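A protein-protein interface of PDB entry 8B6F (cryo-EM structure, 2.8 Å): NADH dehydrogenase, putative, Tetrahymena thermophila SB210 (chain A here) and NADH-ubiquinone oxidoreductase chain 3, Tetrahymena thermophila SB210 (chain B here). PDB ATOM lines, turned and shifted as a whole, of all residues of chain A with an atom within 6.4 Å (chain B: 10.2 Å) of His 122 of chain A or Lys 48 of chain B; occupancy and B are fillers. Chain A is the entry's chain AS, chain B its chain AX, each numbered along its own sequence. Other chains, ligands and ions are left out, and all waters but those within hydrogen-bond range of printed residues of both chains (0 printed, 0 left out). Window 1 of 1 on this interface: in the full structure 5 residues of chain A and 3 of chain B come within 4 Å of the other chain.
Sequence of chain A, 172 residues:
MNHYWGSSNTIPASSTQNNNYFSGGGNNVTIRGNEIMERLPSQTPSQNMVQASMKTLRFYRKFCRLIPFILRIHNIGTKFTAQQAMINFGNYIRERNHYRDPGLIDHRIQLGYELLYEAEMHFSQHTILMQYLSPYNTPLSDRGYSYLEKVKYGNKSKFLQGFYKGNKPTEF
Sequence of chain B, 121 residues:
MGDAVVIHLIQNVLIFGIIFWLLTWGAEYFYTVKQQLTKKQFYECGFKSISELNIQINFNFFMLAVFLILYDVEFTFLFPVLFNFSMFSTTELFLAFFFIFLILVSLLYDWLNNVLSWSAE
Among the printed residues, pairs that only touch across the chains: Met 121 of chain A with Ile 50 of chain B (3.2 Å) and His 122 of chain A with Lys 48 of chain B (3.6 Å).
NH1 of Arg 32 of chain A sits at hydrogen-bond distance from O of Glu 120 of chain A (2.7 Å).
Of chain B, only Lys 48 (3.6 Å) comes within 4 Å of His 122 of chain A. Of the printed residues of chain A, Lys 48 of chain B touches Ile 73 (3.3 Å) and His 122 (3.6 Å). Of the printed residues of chain B, Ile 73 of chain A touches Lys 48 (3.3 Å). No residue of chain B comes within 4 Å of His 74 of chain A. No residue of chain B comes within 4 Å of Ala 119 of chain A. Printed residues of chain B within 4 Å of Met 121 of chain A: Ile 50 (3.2 Å). Of the printed residues of chain B, Arg 32 of chain A touches Ile 50. The nearest residue of chain B that does not touch His 122 of chain A is Ile 50 of chain B (4.1 Å). The nearest printed residue of chain B that does not touch Arg 32 of chain A is Ser 51 of chain B (4.1 Å).
The guanidinium group of Arg 32 of chain A lies within hydrogen-bond range of the backbone carbonyl oxygen of Ile 50 of chain B (2.6 Å). The side-chain amino group of Lys 48 of chain B lies within hydrogen-bond range of the backbone carbonyl oxygen of Ile 73 of chain A, at 3.3 Å.
Hydrophobic or aromatic side chains of chain A within 4 Å of the printed part of chain B: His 122. Printed residues of chain B that touch a printed residue of chain A: Lys 48 and Ile 50.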
ATOM      1  N   ARG A  32      -3.760  -8.377  -7.632  1.00  0.00           N
ATOM      2  CA  ARG A  32      -3.867  -9.151  -6.405  1.00  0.00           C
ATOM      3  C   ARG A  32      -2.957  -8.577  -5.325  1.00  0.00           C
ATOM      4  O   ARG A  32      -1.920  -7.972  -5.608  1.00  0.00           O
ATOM      5  CB  ARG A  32      -3.519 -10.618  -6.658  1.00  0.00           C
ATOM      6  CG  ARG A  32      -2.170 -10.845  -7.317  1.00  0.00           C
ATOM      7  CD  ARG A  32      -1.740 -12.296  -7.176  1.00  0.00           C
ATOM      8  NE  ARG A  32      -0.609 -12.617  -8.036  1.00  0.00           N
ATOM      9  CZ  ARG A  32      -0.705 -13.149  -9.248  1.00  0.00           C
ATOM     10  NH1 ARG A  32      -1.877 -13.447  -9.784  1.00  0.00           N
ATOM     11  NH2 ARG A  32       0.404 -13.384  -9.941  1.00  0.00           N
ATOM     12  N   ILE A  70      -6.881  -9.737 -15.062  1.00  0.00           N
ATOM     13  CA  ILE A  70      -7.227 -11.136 -15.300  1.00  0.00           C
ATOM     14  C   ILE A  70      -6.925 -11.515 -16.743  1.00  0.00           C
ATOM     15  O   ILE A  70      -6.325 -12.559 -17.018  1.00  0.00           O
ATOM     16  CB  ILE A  70      -8.703 -11.389 -14.946  1.00  0.00           C
ATOM     17  CG1 ILE A  70      -8.946 -11.078 -13.466  1.00  0.00           C
ATOM     18  CG2 ILE A  70      -9.091 -12.828 -15.257  1.00  0.00           C
ATOM     19  CD1 ILE A  70     -10.397 -11.175 -13.035  1.00  0.00           C
ATOM     20  N   ILE A  73      -3.047 -11.757 -17.377  1.00  0.00           N
ATOM     21  CA  ILE A  73      -2.365 -12.905 -16.787  1.00  0.00           C
ATOM     22  C   ILE A  73      -2.789 -14.199 -17.472  1.00  0.00           C
ATOM     23  O   ILE A  73      -1.971 -15.103 -17.674  1.00  0.00           O
ATOM     24  CB  ILE A  73      -2.601 -12.961 -15.264  1.00  0.00           C
ATOM     25  CG1 ILE A  73      -4.086 -13.155 -14.942  1.00  0.00           C
ATOM     26  CG2 ILE A  73      -2.050 -11.704 -14.607  1.00  0.00           C
ATOM     27  CD1 ILE A  73      -4.392 -13.268 -13.457  1.00  0.00           C
ATOM     28  N   HIS A  74      -4.065 -14.316 -17.840  1.00  0.00           N
ATOM     29  CA  HIS A  74      -4.572 -15.542 -18.441  1.00  0.00           C
ATOM     30  C   HIS A  74      -4.402 -15.586 -19.953  1.00  0.00           C
ATOM     31  O   HIS A  74      -4.741 -16.602 -20.567  1.00  0.00           O
ATOM     32  CB  HIS A  74      -6.053 -15.728 -18.096  1.00  0.00           C
ATOM     33  CG  HIS A  74      -6.295 -16.078 -16.662  1.00  0.00           C
ATOM     34  ND1 HIS A  74      -6.045 -17.333 -16.150  1.00  0.00           N
ATOM     35  CD2 HIS A  74      -6.765 -15.339 -15.631  1.00  0.00           C
ATOM     36  CE1 HIS A  74      -6.347 -17.350 -14.865  1.00  0.00           C
ATOM     37  NE2 HIS A  74      -6.787 -16.153 -14.525  1.00  0.00           N
ATOM     38  N   ASN A  75      -3.886 -14.524 -20.569  1.00  0.00           N
ATOM     39  CA  ASN A  75      -3.628 -14.511 -22.007  1.00  0.00           C
ATOM     40  C   ASN A  75      -4.909 -14.764 -22.802  1.00  0.00           C
ATOM     41  O   ASN A  75      -4.920 -15.521 -23.774  1.00  0.00           O
ATOM     42  CB  ASN A  75      -2.548 -15.532 -22.375  1.00  0.00           C
ATOM     43  CG  ASN A  75      -2.152 -15.463 -23.835  1.00  0.00           C
ATOM     44  OD1 ASN A  75      -2.212 -14.405 -24.456  1.00  0.00           O
ATOM     45  ND2 ASN A  75      -1.749 -16.598 -24.391  1.00  0.00           N
ATOM     46  N   TYR A 117     -11.564 -14.121  -6.854  1.00  0.00           N
ATOM     47  CA  TYR A 117     -10.273 -14.350  -6.215  1.00  0.00           C
ATOM     48  C   TYR A 117      -9.537 -15.511  -6.867  1.00  0.00           C
ATOM     49  O   TYR A 117      -8.318 -15.452  -7.068  1.00  0.00           O
ATOM     50  CB  TYR A 117     -10.466 -14.609  -4.723  1.00  0.00           C
ATOM     51  CG  TYR A 117      -9.188 -14.946  -3.996  1.00  0.00           C
ATOM     52  CD1 TYR A 117      -8.330 -13.946  -3.561  1.00  0.00           C
ATOM     53  CD2 TYR A 117      -8.842 -16.264  -3.737  1.00  0.00           C
ATOM     54  CE1 TYR A 117      -7.164 -14.250  -2.894  1.00  0.00           C
ATOM     55  CE2 TYR A 117      -7.676 -16.577  -3.069  1.00  0.00           C
ATOM     56  CZ  TYR A 117      -6.843 -15.564  -2.649  1.00  0.00           C
ATOM     57  OH  TYR A 117      -5.680 -15.871  -1.984  1.00  0.00           O
ATOM     58  N   GLU A 118     -10.257 -16.582  -7.202  1.00  0.00           N
ATOM     59  CA  GLU A 118      -9.633 -17.702  -7.897  1.00  0.00           C
ATOM     60  C   GLU A 118      -9.039 -17.256  -9.225  1.00  0.00           C
ATOM     61  O   GLU A 118      -7.913 -17.633  -9.568  1.00  0.00           O
ATOM     62  CB  GLU A 118     -10.653 -18.818  -8.116  1.00  0.00           C
ATOM     63  CG  GLU A 118     -11.131 -19.477  -6.836  1.00  0.00           C
ATOM     64  CD  GLU A 118     -12.239 -20.480  -7.083  1.00  0.00           C
ATOM     65  OE1 GLU A 118     -12.597 -20.689  -8.260  1.00  0.00           O
ATOM     66  OE2 GLU A 118     -12.750 -21.060  -6.102  1.00  0.00           O
ATOM     67  N   ALA A 119      -9.783 -16.458  -9.990  1.00  0.00           N
ATOM     68  CA  ALA A 119      -9.266 -15.963 -11.262  1.00  0.00           C
ATOM     69  C   ALA A 119      -8.014 -15.119 -11.057  1.00  0.00           C
ATOM     70  O   ALA A 119      -7.046 -15.239 -11.817  1.00  0.00           O
ATOM     71  CB  ALA A 119     -10.343 -15.156 -11.985  1.00  0.00           C
ATOM     72  N   GLU A 120      -8.010 -14.263 -10.033  1.00  0.00           N
ATOM     73  CA  GLU A 120      -6.826 -13.457  -9.744  1.00  0.00           C
ATOM     74  C   GLU A 120      -5.620 -14.333  -9.437  1.00  0.00           C
ATOM     75  O   GLU A 120      -4.515 -14.082  -9.932  1.00  0.00           O
ATOM     76  CB  GLU A 120      -7.091 -12.533  -8.556  1.00  0.00           C
ATOM     77  CG  GLU A 120      -8.189 -11.513  -8.751  1.00  0.00           C
ATOM     78  CD  GLU A 120      -8.563 -10.838  -7.446  1.00  0.00           C
ATOM     79  OE1 GLU A 120      -7.643 -10.458  -6.692  1.00  0.00           O
ATOM     80  OE2 GLU A 120      -9.771 -10.702  -7.164  1.00  0.00           O
ATOM     81  N   MET A 121      -5.809 -15.363  -8.620  1.00  0.00           N
ATOM     82  CA  MET A 121      -4.718 -16.176  -8.106  1.00  0.00           C
ATOM     83  C   MET A 121      -4.391 -17.369  -8.991  1.00  0.00           C
ATOM     84  O   MET A 121      -3.584 -18.214  -8.591  1.00  0.00           O
ATOM     85  CB  MET A 121      -5.054 -16.663  -6.695  1.00  0.00           C
ATOM     86  CG  MET A 121      -4.914 -15.601  -5.623  1.00  0.00           C
ATOM     87  SD  MET A 121      -3.208 -15.074  -5.378  1.00  0.00           S
ATOM     88  CE  MET A 121      -3.404 -13.924  -4.020  1.00  0.00           C
ATOM     89  N   HIS A 122      -4.999 -17.469 -10.171  1.00  0.00           N
ATOM     90  CA  HIS A 122      -4.715 -18.532 -11.129  1.00  0.00           C
ATOM     91  C   HIS A 122      -5.170 -19.896 -10.631  1.00  0.00           C
ATOM     92  O   HIS A 122      -4.708 -20.926 -11.133  1.00  0.00           O
ATOM     93  CB  HIS A 122      -3.223 -18.587 -11.488  1.00  0.00           C
ATOM     94  CG  HIS A 122      -2.854 -17.738 -12.663  1.00  0.00           C
ATOM     95  ND1 HIS A 122      -3.175 -18.081 -13.959  1.00  0.00           N
ATOM     96  CD2 HIS A 122      -2.176 -16.569 -12.741  1.00  0.00           C
ATOM     97  CE1 HIS A 122      -2.719 -17.156 -14.782  1.00  0.00           C
ATOM     98  NE2 HIS A 122      -2.109 -16.227 -14.069  1.00  0.00           N
ATOM     99  N   PHE A 123      -6.067 -19.934  -9.643  1.00  0.00           N
ATOM    100  CA  PHE A 123      -6.601 -21.212  -9.193  1.00  0.00           C
ATOM    101  C   PHE A 123      -7.360 -21.910 -10.314  1.00  0.00           C
ATOM    102  O   PHE A 123      -7.312 -23.139 -10.435  1.00  0.00           O
ATOM    103  CB  PHE A 123      -7.509 -21.006  -7.978  1.00  0.00           C
ATOM    104  CG  PHE A 123      -6.796 -20.483  -6.759  1.00  0.00           C
ATOM    105  CD1 PHE A 123      -5.411 -20.483  -6.682  1.00  0.00           C
ATOM    106  CD2 PHE A 123      -7.517 -20.000  -5.683  1.00  0.00           C
ATOM    107  CE1 PHE A 123      -4.765 -20.007  -5.558  1.00  0.00           C
ATOM    108  CE2 PHE A 123      -6.876 -19.522  -4.557  1.00  0.00           C
ATOM    109  CZ  PHE A 123      -5.499 -19.526  -4.495  1.00  0.00           C
ATOM    110  N   SER A 124      -8.059 -21.145 -11.144  1.00  0.00           N
ATOM    111  CA  SER A 124      -8.812 -21.679 -12.267  1.00  0.00           C
ATOM    112  C   SER A 124      -7.998 -21.581 -13.552  1.00  0.00           C
ATOM    113  O   SER A 124      -7.013 -20.845 -13.640  1.00  0.00           O
ATOM    114  CB  SER A 124     -10.136 -20.930 -12.433  1.00  0.00           C
ATOM    115  OG  SER A 124     -10.826 -20.832 -11.199  1.00  0.00           O
ATOM    116  N   GLN A 125      -8.420 -22.346 -14.553  1.00  0.00           N
ATOM    117  CA  GLN A 125      -7.807 -22.305 -15.872  1.00  0.00           C
ATOM    118  C   GLN A 125      -8.533 -21.290 -16.745  1.00  0.00           C
ATOM    119  O   GLN A 125      -9.721 -21.021 -16.558  1.00  0.00           O
ATOM    120  CB  GLN A 125      -7.843 -23.685 -16.530  1.00  0.00           C
ATOM    121  CG  GLN A 125      -6.958 -23.810 -17.757  1.00  0.00           C
ATOM    122  CD  GLN A 125      -5.487 -23.683 -17.428  1.00  0.00           C
ATOM    123  OE1 GLN A 125      -5.076 -23.891 -16.289  1.00  0.00           O
ATOM    124  NE2 GLN A 125      -4.686 -23.336 -18.426  1.00  0.00           N
ATOM    125  N   LEU B  37       1.256 -25.813 -25.057  1.00  0.00           N
ATOM    126  CA  LEU B  37       1.034 -24.541 -24.375  1.00  0.00           C
ATOM    127  C   LEU B  37       1.930 -24.396 -23.153  1.00  0.00           C
ATOM    128  O   LEU B  37       2.643 -23.398 -23.008  1.00  0.00           O
ATOM    129  CB  LEU B  37      -0.438 -24.418 -23.983  1.00  0.00           C
ATOM    130  CG  LEU B  37      -0.845 -23.132 -23.261  1.00  0.00           C
ATOM    131  CD1 LEU B  37      -0.526 -21.909 -24.104  1.00  0.00           C
ATOM    132  CD2 LEU B  37      -2.324 -23.166 -22.908  1.00  0.00           C
ATOM    133  N   THR B  38       1.915 -25.386 -22.265  1.00  0.00           N
ATOM    134  CA  THR B  38       2.609 -25.303 -20.988  1.00  0.00           C
ATOM    135  C   THR B  38       3.937 -26.049 -20.983  1.00  0.00           C
ATOM    136  O   THR B  38       4.525 -26.239 -19.914  1.00  0.00           O
ATOM    137  CB  THR B  38       1.717 -25.836 -19.868  1.00  0.00           C
ATOM    138  OG1 THR B  38       1.569 -27.252 -20.011  1.00  0.00           O
ATOM    139  CG2 THR B  38       0.343 -25.182 -19.910  1.00  0.00           C
ATOM    140  N   LYS B  40       6.831 -25.119 -22.066  1.00  0.00           N
ATOM    141  CA  LYS B  40       7.956 -24.227 -21.814  1.00  0.00           C
ATOM    142  C   LYS B  40       7.581 -23.148 -20.808  1.00  0.00           C
ATOM    143  O   LYS B  40       7.900 -21.971 -20.983  1.00  0.00           O
ATOM    144  CB  LYS B  40       8.446 -23.594 -23.114  1.00  0.00           C
ATOM    145  CG  LYS B  40       8.910 -24.593 -24.158  1.00  0.00           C
ATOM    146  CD  LYS B  40       9.402 -23.887 -25.411  1.00  0.00           C
ATOM    147  CE  LYS B  40       9.926 -24.874 -26.441  1.00  0.00           C
ATOM    148  NZ  LYS B  40       8.873 -25.817 -26.909  1.00  0.00           N
ATOM    149  N   GLN B  41       6.896 -23.540 -19.738  1.00  0.00           N
ATOM    150  CA  GLN B  41       6.501 -22.632 -18.674  1.00  0.00           C
ATOM    151  C   GLN B  41       7.051 -23.130 -17.344  1.00  0.00           C
ATOM    152  O   GLN B  41       7.468 -24.284 -17.212  1.00  0.00           O
ATOM    153  CB  GLN B  41       4.977 -22.494 -18.597  1.00  0.00           C
ATOM    154  CG  GLN B  41       4.361 -21.872 -19.840  1.00  0.00           C
ATOM    155  CD  GLN B  41       2.873 -21.634 -19.699  1.00  0.00           C
ATOM    156  OE1 GLN B  41       2.260 -22.030 -18.709  1.00  0.00           O
ATOM    157  NE2 GLN B  41       2.283 -20.981 -20.692  1.00  0.00           N
ATOM    158  N   PHE B  42       7.050 -22.242 -16.356  1.00  0.00           N
ATOM    159  CA  PHE B  42       7.616 -22.575 -15.056  1.00  0.00           C
ATOM    160  C   PHE B  42       6.820 -23.694 -14.393  1.00  0.00           C
ATOM    161  O   PHE B  42       5.588 -23.721 -14.447  1.00  0.00           O
ATOM    162  CB  PHE B  42       7.639 -21.342 -14.155  1.00  0.00           C
ATOM    163  CG  PHE B  42       8.448 -20.207 -14.708  1.00  0.00           C
ATOM    164  CD1 PHE B  42       9.802 -20.361 -14.953  1.00  0.00           C
ATOM    165  CD2 PHE B  42       7.859 -18.982 -14.966  1.00  0.00           C
ATOM    166  CE1 PHE B  42      10.550 -19.318 -15.458  1.00  0.00           C
ATOM    167  CE2 PHE B  42       8.600 -17.934 -15.470  1.00  0.00           C
ATOM    168  CZ  PHE B  42       9.949 -18.102 -15.716  1.00  0.00           C
ATOM    169  N   TYR B  43       7.539 -24.616 -13.760  1.00  0.00           N
ATOM    170  CA  TYR B  43       6.932 -25.751 -13.079  1.00  0.00           C
ATOM    171  C   TYR B  43       6.672 -25.387 -11.622  1.00  0.00           C
ATOM    172  O   TYR B  43       7.593 -24.986 -10.902  1.00  0.00           O
ATOM    173  CB  TYR B  43       7.842 -26.975 -13.179  1.00  0.00           C
ATOM    174  CG  TYR B  43       7.536 -28.051 -12.166  1.00  0.00           C
ATOM    175  CD1 TYR B  43       6.503 -28.953 -12.372  1.00  0.00           C
ATOM    176  CD2 TYR B  43       8.287 -28.169 -11.006  1.00  0.00           C
ATOM    177  CE1 TYR B  43       6.225 -29.940 -11.450  1.00  0.00           C
ATOM    178  CE2 TYR B  43       8.016 -29.150 -10.077  1.00  0.00           C
ATOM    179  CZ  TYR B  43       6.985 -30.033 -10.305  1.00  0.00           C
ATOM    180  OH  TYR B  43       6.712 -31.013  -9.381  1.00  0.00           O
ATOM    181  N   GLU B  44       5.421 -25.530 -11.190  1.00  0.00           N
ATOM    182  CA  GLU B  44       4.994 -25.221  -9.829  1.00  0.00           C
ATOM    183  C   GLU B  44       4.120 -26.345  -9.287  1.00  0.00           C
ATOM    184  O   GLU B  44       3.033 -26.123  -8.750  1.00  0.00           O
ATOM    185  CB  GLU B  44       4.253 -23.889  -9.783  1.00  0.00           C
ATOM    186  CG  GLU B  44       4.028 -23.337  -8.382  1.00  0.00           C
ATOM    187  CD  GLU B  44       5.299 -22.814  -7.743  1.00  0.00           C
ATOM    188  OE1 GLU B  44       6.367 -22.892  -8.384  1.00  0.00           O
ATOM    189  OE2 GLU B  44       5.226 -22.320  -6.599  1.00  0.00           O
ATOM    190  N   CYS B  45       4.587 -27.583  -9.446  1.00  0.00           N
ATOM    191  CA  CYS B  45       3.889 -28.764  -8.937  1.00  0.00           C
ATOM    192  C   CYS B  45       2.544 -28.956  -9.636  1.00  0.00           C
ATOM    193  O   CYS B  45       1.518 -29.206  -9.004  1.00  0.00           O
ATOM    194  CB  CYS B  45       3.705 -28.682  -7.418  1.00  0.00           C
ATOM    195  SG  CYS B  45       5.242 -28.653  -6.475  1.00  0.00           S
ATOM    196  N   GLY B  46       2.557 -28.840 -10.961  1.00  0.00           N
ATOM    197  CA  GLY B  46       1.372 -29.133 -11.741  1.00  0.00           C
ATOM    198  C   GLY B  46       0.364 -28.013 -11.838  1.00  0.00           C
ATOM    199  O   GLY B  46      -0.800 -28.274 -12.152  1.00  0.00           O
ATOM    200  N   PHE B  47       0.764 -26.774 -11.574  1.00  0.00           N
ATOM    201  CA  PHE B  47      -0.128 -25.636 -11.733  1.00  0.00           C
ATOM    202  C   PHE B  47       0.697 -24.421 -12.125  1.00  0.00           C
ATOM    203  O   PHE B  47       1.908 -24.373 -11.905  1.00  0.00           O
ATOM    204  CB  PHE B  47      -0.933 -25.366 -10.457  1.00  0.00           C
ATOM    205  CG  PHE B  47      -2.102 -26.294 -10.274  1.00  0.00           C
ATOM    206  CD1 PHE B  47      -3.314 -26.032 -10.893  1.00  0.00           C
ATOM    207  CD2 PHE B  47      -1.989 -27.426  -9.486  1.00  0.00           C
ATOM    208  CE1 PHE B  47      -4.393 -26.883 -10.729  1.00  0.00           C
ATOM    209  CE2 PHE B  47      -3.064 -28.280  -9.317  1.00  0.00           C
ATOM    210  CZ  PHE B  47      -4.268 -28.007  -9.942  1.00  0.00           C
ATOM    211  N   LYS B  48       0.027 -23.440 -12.721  1.00  0.00           N
ATOM    212  CA  LYS B  48       0.724 -22.263 -13.213  1.00  0.00           C
ATOM    213  C   LYS B  48       1.245 -21.427 -12.050  1.00  0.00           C
ATOM    214  O   LYS B  48       0.544 -21.207 -11.059  1.00  0.00           O
ATOM    215  CB  LYS B  48      -0.204 -21.428 -14.091  1.00  0.00           C
ATOM    216  CG  LYS B  48       0.499 -20.323 -14.856  1.00  0.00           C
ATOM    217  CD  LYS B  48      -0.407 -19.731 -15.921  1.00  0.00           C
ATOM    218  CE  LYS B  48       0.302 -18.640 -16.704  1.00  0.00           C
ATOM    219  NZ  LYS B  48      -0.561 -18.076 -17.781  1.00  0.00           N
ATOM    220  N   SER B  49       2.484 -20.959 -12.178  1.00  0.00           N
ATOM    221  CA  SER B  49       3.088 -20.116 -11.156  1.00  0.00           C
ATOM    222  C   SER B  49       2.540 -18.701 -11.270  1.00  0.00           C
ATOM    223  O   SER B  49       2.553 -18.105 -12.352  1.00  0.00           O
ATOM    224  CB  SER B  49       4.610 -20.111 -11.296  1.00  0.00           C
ATOM    225  OG  SER B  49       4.998 -19.671 -12.584  1.00  0.00           O
ATOM    226  N   ILE B  50       2.060 -18.160 -10.151  1.00  0.00           N
ATOM    227  CA  ILE B  50       1.427 -16.846 -10.186  1.00  0.00           C
ATOM    228  C   ILE B  50       2.462 -15.757 -10.432  1.00  0.00           C
ATOM    229  O   ILE B  50       2.214 -14.809 -11.188  1.00  0.00           O
ATOM    230  CB  ILE B  50       0.627 -16.592  -8.894  1.00  0.00           C
ATOM    231  CG1 ILE B  50       1.562 -16.465  -7.687  1.00  0.00           C
ATOM    232  CG2 ILE B  50      -0.389 -17.710  -8.687  1.00  0.00           C
ATOM    233  CD1 ILE B  50       0.847 -16.258  -6.372  1.00  0.00           C
ATOM    234  N   SER B  51       3.632 -15.868  -9.810  1.00  0.00           N
ATOM    235  CA  SER B  51       4.649 -14.829  -9.859  1.00  0.00           C
ATOM    236  C   SER B  51       5.935 -15.381 -10.452  1.00  0.00           C
ATOM    237  O   SER B  51       6.349 -16.499 -10.134  1.00  0.00           O
ATOM    238  CB  SER B  51       4.925 -14.271  -8.458  1.00  0.00           C
ATOM    239  OG  SER B  51       5.937 -13.280  -8.491  1.00  0.00           O
ATOM    240  N   GLU B  52       6.566 -14.586 -11.313  1.00  0.00           N
ATOM    241  CA  GLU B  52       7.860 -14.924 -11.884  1.00  0.00           C
ATOM    242  C   GLU B  52       8.711 -13.666 -11.961  1.00  0.00           C
ATOM    243  O   GLU B  52       8.233 -12.607 -12.373  1.00  0.00           O
ATOM    244  CB  GLU B  52       7.713 -15.556 -13.273  1.00  0.00           C
ATOM    245  CG  GLU B  52       7.399 -14.571 -14.391  1.00  0.00           C
ATOM    246  CD  GLU B  52       8.644 -13.998 -15.046  1.00  0.00           C
ATOM    247  OE1 GLU B  52       9.763 -14.356 -14.623  1.00  0.00           O
ATOM    248  OE2 GLU B  52       8.503 -13.191 -15.988  1.00  0.00           O
